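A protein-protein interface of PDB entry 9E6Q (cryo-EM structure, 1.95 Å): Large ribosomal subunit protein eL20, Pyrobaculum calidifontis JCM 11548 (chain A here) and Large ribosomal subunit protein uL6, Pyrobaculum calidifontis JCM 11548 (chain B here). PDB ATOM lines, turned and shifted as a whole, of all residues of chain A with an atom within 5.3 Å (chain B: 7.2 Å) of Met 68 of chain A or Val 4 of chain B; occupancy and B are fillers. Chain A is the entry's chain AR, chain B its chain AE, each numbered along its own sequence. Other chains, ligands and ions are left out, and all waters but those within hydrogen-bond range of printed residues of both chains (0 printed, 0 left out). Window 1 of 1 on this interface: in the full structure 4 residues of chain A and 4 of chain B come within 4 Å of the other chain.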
ATOM      1  N   ASN A  64      22.185 -14.052  17.404  1.00  0.00           N
ATOM      2  CA  ASN A  64      22.287 -13.087  16.318  1.00  0.00           C
ATOM      3  C   ASN A  64      22.548 -13.769  14.988  1.00  0.00           C
ATOM      4  O   ASN A  64      22.209 -13.216  13.937  1.00  0.00           O
ATOM      5  CB  ASN A  64      23.386 -12.072  16.615  1.00  0.00           C
ATOM      6  CG  ASN A  64      23.196 -11.387  17.946  1.00  0.00           C
ATOM      7  OD1 ASN A  64      22.124 -10.855  18.234  1.00  0.00           O
ATOM      8  ND2 ASN A  64      24.236 -11.392  18.769  1.00  0.00           N
ATOM      9  N   GLU A  65      23.155 -14.954  15.013  1.00  0.00           N
ATOM     10  CA  GLU A  65      23.284 -15.744  13.797  1.00  0.00           C
ATOM     11  C   GLU A  65      21.916 -16.016  13.189  1.00  0.00           C
ATOM     12  O   GLU A  65      21.691 -15.772  12.000  1.00  0.00           O
ATOM     13  CB  GLU A  65      24.006 -17.057  14.101  1.00  0.00           C
ATOM     14  CG  GLU A  65      24.575 -17.755  12.881  1.00  0.00           C
ATOM     15  CD  GLU A  65      25.638 -18.776  13.236  1.00  0.00           C
ATOM     16  OE1 GLU A  65      26.195 -18.701  14.352  1.00  0.00           O
ATOM     17  OE2 GLU A  65      25.921 -19.654  12.395  1.00  0.00           O
ATOM     18  N   ALA A  66      20.978 -16.496  14.003  1.00  0.00           N
ATOM     19  CA  ALA A  66      19.653 -16.823  13.492  1.00  0.00           C
ATOM     20  C   ALA A  66      18.947 -15.584  12.964  1.00  0.00           C
ATOM     21  O   ALA A  66      18.320 -15.621  11.901  1.00  0.00           O
ATOM     22  CB  ALA A  66      18.824 -17.497  14.582  1.00  0.00           C
ATOM     23  N   LYS A  67      19.042 -14.471  13.693  1.00  0.00           N
ATOM     24  CA  LYS A  67      18.404 -13.236  13.248  1.00  0.00           C
ATOM     25  C   LYS A  67      18.965 -12.778  11.910  1.00  0.00           C
ATOM     26  O   LYS A  67      18.216 -12.391  11.009  1.00  0.00           O
ATOM     27  CB  LYS A  67      18.588 -12.141  14.292  1.00  0.00           C
ATOM     28  CG  LYS A  67      17.709 -12.266  15.503  1.00  0.00           C
ATOM     29  CD  LYS A  67      18.475 -11.849  16.731  1.00  0.00           C
ATOM     30  CE  LYS A  67      17.597 -11.855  17.953  1.00  0.00           C
ATOM     31  NZ  LYS A  67      17.495 -10.491  18.545  1.00  0.00           N
ATOM     32  N   MET A  68      20.289 -12.816  11.763  1.00  0.00           N
ATOM     33  CA  MET A  68      20.911 -12.323  10.542  1.00  0.00           C
ATOM     34  C   MET A  68      20.553 -13.192   9.344  1.00  0.00           C
ATOM     35  O   MET A  68      20.397 -12.683   8.230  1.00  0.00           O
ATOM     36  CB  MET A  68      22.424 -12.249  10.720  1.00  0.00           C
ATOM     37  CG  MET A  68      22.922 -10.919  11.238  1.00  0.00           C
ATOM     38  SD  MET A  68      24.684 -10.702  10.946  1.00  0.00           S
ATOM     39  CE  MET A  68      25.355 -11.398  12.452  1.00  0.00           C
ATOM     40  N   LEU A  69      20.430 -14.506   9.545  1.00  0.00           N
ATOM     41  CA  LEU A  69      20.016 -15.374   8.445  1.00  0.00           C
ATOM     42  C   LEU A  69      18.602 -15.049   7.986  1.00  0.00           C
ATOM     43  O   LEU A  69      18.299 -15.130   6.793  1.00  0.00           O
ATOM     44  CB  LEU A  69      20.115 -16.843   8.852  1.00  0.00           C
ATOM     45  CG  LEU A  69      21.490 -17.366   9.248  1.00  0.00           C
ATOM     46  CD1 LEU A  69      21.377 -18.779   9.782  1.00  0.00           C
ATOM     47  CD2 LEU A  69      22.433 -17.314   8.070  1.00  0.00           C
ATOM     48  N   MET A  70      17.731 -14.661   8.917  1.00  0.00           N
ATOM     49  CA  MET A  70      16.336 -14.408   8.579  1.00  0.00           C
ATOM     50  C   MET A  70      16.170 -13.292   7.561  1.00  0.00           C
ATOM     51  O   MET A  70      15.230 -13.321   6.763  1.00  0.00           O
ATOM     52  CB  MET A  70      15.552 -14.070   9.838  1.00  0.00           C
ATOM     53  CG  MET A  70      15.225 -15.258  10.672  1.00  0.00           C
ATOM     54  SD  MET A  70      14.605 -16.586   9.638  1.00  0.00           S
ATOM     55  CE  MET A  70      12.937 -16.656  10.248  1.00  0.00           C
ATOM     56  N   VAL A  71      17.054 -12.299   7.576  1.00  0.00           N
ATOM     57  CA  VAL A  71      16.920 -11.131   6.718  1.00  0.00           C
ATOM     58  C   VAL A  71      17.867 -11.188   5.529  1.00  0.00           C
ATOM     59  O   VAL A  71      18.022 -10.192   4.818  1.00  0.00           O
ATOM     60  CB  VAL A  71      17.119  -9.834   7.512  1.00  0.00           C
ATOM     61  CG1 VAL A  71      16.186  -9.805   8.700  1.00  0.00           C
ATOM     62  CG2 VAL A  71      18.553  -9.717   7.972  1.00  0.00           C
ATOM     63  N   LEU A  72      18.503 -12.332   5.293  1.00  0.00           N
ATOM     64  CA  LEU A  72      19.442 -12.455   4.188  1.00  0.00           C
ATOM     65  C   LEU A  72      18.732 -12.249   2.858  1.00  0.00           C
ATOM     66  O   LEU A  72      17.652 -12.797   2.625  1.00  0.00           O
ATOM     67  CB  LEU A  72      20.109 -13.828   4.223  1.00  0.00           C
ATOM     68  CG  LEU A  72      21.635 -13.860   4.212  1.00  0.00           C
ATOM     69  CD1 LEU A  72      22.183 -12.723   5.048  1.00  0.00           C
ATOM     70  CD2 LEU A  72      22.127 -15.190   4.730  1.00  0.00           C
ATOM     71  N   HIS B   2      30.913 -17.618  14.816  1.00  0.00           N
ATOM     72  CA  HIS B   2      30.598 -17.531  13.400  1.00  0.00           C
ATOM     73  C   HIS B   2      29.816 -16.259  13.127  1.00  0.00           C
ATOM     74  O   HIS B   2      28.891 -15.919  13.868  1.00  0.00           O
ATOM     75  CB  HIS B   2      29.784 -18.727  12.926  1.00  0.00           C
ATOM     76  CG  HIS B   2      29.261 -18.571  11.537  1.00  0.00           C
ATOM     77  ND1 HIS B   2      27.976 -18.156  11.268  1.00  0.00           N
ATOM     78  CD2 HIS B   2      29.855 -18.760  10.336  1.00  0.00           C
ATOM     79  CE1 HIS B   2      27.798 -18.102   9.961  1.00  0.00           C
ATOM     80  NE2 HIS B   2      28.923 -18.463   9.373  1.00  0.00           N
ATOM     81  N   VAL B   3      30.175 -15.579  12.046  1.00  0.00           N
ATOM     82  CA  VAL B   3      29.612 -14.283  11.696  1.00  0.00           C
ATOM     83  C   VAL B   3      28.895 -14.423  10.367  1.00  0.00           C
ATOM     84  O   VAL B   3      29.513 -14.789   9.361  1.00  0.00           O
ATOM     85  CB  VAL B   3      30.694 -13.197  11.611  1.00  0.00           C
ATOM     86  CG1 VAL B   3      30.085 -11.887  11.183  1.00  0.00           C
ATOM     87  CG2 VAL B   3      31.400 -13.047  12.938  1.00  0.00           C
ATOM     88  N   VAL B   4      27.598 -14.130  10.360  1.00  0.00           N
ATOM     89  CA  VAL B   4      26.850 -14.131   9.110  1.00  0.00           C
ATOM     90  C   VAL B   4      27.292 -12.974   8.231  1.00  0.00           C
ATOM     91  O   VAL B   4      27.574 -13.145   7.041  1.00  0.00           O
ATOM     92  CB  VAL B   4      25.340 -14.074   9.390  1.00  0.00           C
ATOM     93  CG1 VAL B   4      24.575 -13.824   8.109  1.00  0.00           C
ATOM     94  CG2 VAL B   4      24.887 -15.350  10.055  1.00  0.00           C
ATOM     95  N   TYR B   5      27.368 -11.781   8.807  1.00  0.00           N
ATOM     96  CA  TYR B   5      27.744 -10.596   8.059  1.00  0.00           C
ATOM     97  C   TYR B   5      28.279  -9.563   9.038  1.00  0.00           C
ATOM     98  O   TYR B   5      27.737  -9.399  10.132  1.00  0.00           O
ATOM     99  CB  TYR B   5      26.553 -10.039   7.277  1.00  0.00           C
ATOM    100  CG  TYR B   5      26.719  -8.609   6.836  1.00  0.00           C
ATOM    101  CD1 TYR B   5      26.201  -7.565   7.587  1.00  0.00           C
ATOM    102  CD2 TYR B   5      27.387  -8.303   5.664  1.00  0.00           C
ATOM    103  CE1 TYR B   5      26.353  -6.260   7.182  1.00  0.00           C
ATOM    104  CE2 TYR B   5      27.539  -7.006   5.251  1.00  0.00           C
ATOM    105  CZ  TYR B   5      27.022  -5.988   6.011  1.00  0.00           C
ATOM    106  OH  TYR B   5      27.178  -4.690   5.595  1.00  0.00           O
ATOM    107  N   ALA B   6      29.341  -8.875   8.637  1.00  0.00           N
ATOM    108  CA  ALA B   6      29.941  -7.841   9.463  1.00  0.00           C
ATOM    109  C   ALA B   6      30.507  -6.769   8.552  1.00  0.00           C
ATOM    110  O   ALA B   6      31.024  -7.073   7.477  1.00  0.00           O
ATOM    111  CB  ALA B   6      31.036  -8.411  10.366  1.00  0.00           C
ATOM    112  N   VAL B  61      32.862  -8.653   5.552  1.00  0.00           N
ATOM    113  CA  VAL B  61      33.097 -10.088   5.474  1.00  0.00           C
ATOM    114  C   VAL B  61      31.745 -10.781   5.499  1.00  0.00           C
ATOM    115  O   VAL B  61      30.828 -10.345   6.200  1.00  0.00           O
ATOM    116  CB  VAL B  61      33.992 -10.607   6.620  1.00  0.00           C
ATOM    117  CG1 VAL B  61      35.431 -10.185   6.409  1.00  0.00           C
ATOM    118  CG2 VAL B  61      33.476 -10.139   7.960  1.00  0.00           C
ATOM    119  N   LEU B  62      31.615 -11.848   4.719  1.00  0.00           N
ATOM    120  CA  LEU B  62      30.404 -12.656   4.676  1.00  0.00           C
ATOM    121  C   LEU B  62      30.733 -14.090   5.051  1.00  0.00           C
ATOM    122  O   LEU B  62      31.762 -14.622   4.634  1.00  0.00           O
ATOM    123  CB  LEU B  62      29.760 -12.629   3.298  1.00  0.00           C
ATOM    124  CG  LEU B  62      29.302 -11.266   2.805  1.00  0.00           C
ATOM    125  CD1 LEU B  62      29.169 -11.282   1.304  1.00  0.00           C
ATOM    126  CD2 LEU B  62      27.983 -10.901   3.456  1.00  0.00           C
ATOM    127  N   ASN B  63      29.853 -14.704   5.842  1.00  0.00           N
ATOM    128  CA  ASN B  63      29.973 -16.114   6.209  1.00  0.00           C
ATOM    129  C   ASN B  63      31.341 -16.411   6.822  1.00  0.00           C
ATOM    130  O   ASN B  63      32.023 -17.364   6.448  1.00  0.00           O
ATOM    131  CB  ASN B  63      29.709 -17.007   4.996  1.00  0.00           C
ATOM    132  CG  ASN B  63      29.281 -18.400   5.382  1.00  0.00           C
ATOM    133  OD1 ASN B  63      28.684 -18.607   6.434  1.00  0.00           O
ATOM    134  ND2 ASN B  63      29.583 -19.366   4.532  1.00  0.00           N
ATOM    135  N   ALA B  64      31.731 -15.586   7.784  1.00  0.00           N
ATOM    136  CA  ALA B  64      33.100 -15.535   8.267  1.00  0.00           C
ATOM    137  C   ALA B  64      33.234 -16.175   9.638  1.00  0.00           C
ATOM    138  O   ALA B  64      32.317 -16.130  10.461  1.00  0.00           O
ATOM    139  CB  ALA B  64      33.592 -14.089   8.336  1.00  0.00           C
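OE2 of Glu 65 of chain A lies within hydrogen-bond range of ND1 of His 2 of chain B.
SD of Met 68 of chain A sits at hydrogen-bond distance from N of Tyr 5 of chain B (3.6 Å).
NE2 of His 2 of chain B sits at hydrogen-bond distance from OD1 of Asn 63 of chain B, 3.0 Å away.
The backbone NH (N) of Asn 63 of chain B is in hydrogen-bond range of the backbone carbonyl oxygen (O) of Val 4 of chain B (3.0 Å).
Among the printed residues, pairs that only touch across the chains: Met 68 of chain A with Val 4 of chain B, Leu 69 of chain A with Val 4 of chain B and Glu 65 of chain A with Val 4 of chain B.
Of chain B, only Val 4 (3.7 Å) and Tyr 5 (3.4 Å) come within 4 Å of Met 68 of chain A.
Val 4 of chain B touches just these residues of chain A: Glu 65, Met 68 and Leu 69.
Of the printed residues of chain B, Leu 69 of chain A touches Val 4 (3.7 Å).
Of the printed residues of chain A, His 2 of chain B touches Glu 65.
Of the printed residues of chain B, Glu 65 of chain A touches His 2 and Val 4.
Of the printed residues of chain A, Tyr 5 of chain B touches Met 68 (3.4 Å).
Asn 64 of chain A touches none of the printed residues of chain B.
The nearest printed residue of chain B that does not touch Glu 65 of chain A is Val 3 of chain B (5.6 Å).
Printed residues of chain A that touch a printed residue of chain B: Glu 65, Met 68 and Leu 69.
Printed residues of chain B that touch a printed residue of chain A: His 2, Val 4 and Tyr 5.
Hydrophobic or aromatic side chains of chain B within 4 Å of the printed part of chain A: His 2 and Val 4.
Among the printed residues, no Asp or Glu carboxylate lies within 4 Å of a Lys or Arg side-chain nitrogen of the other chain.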
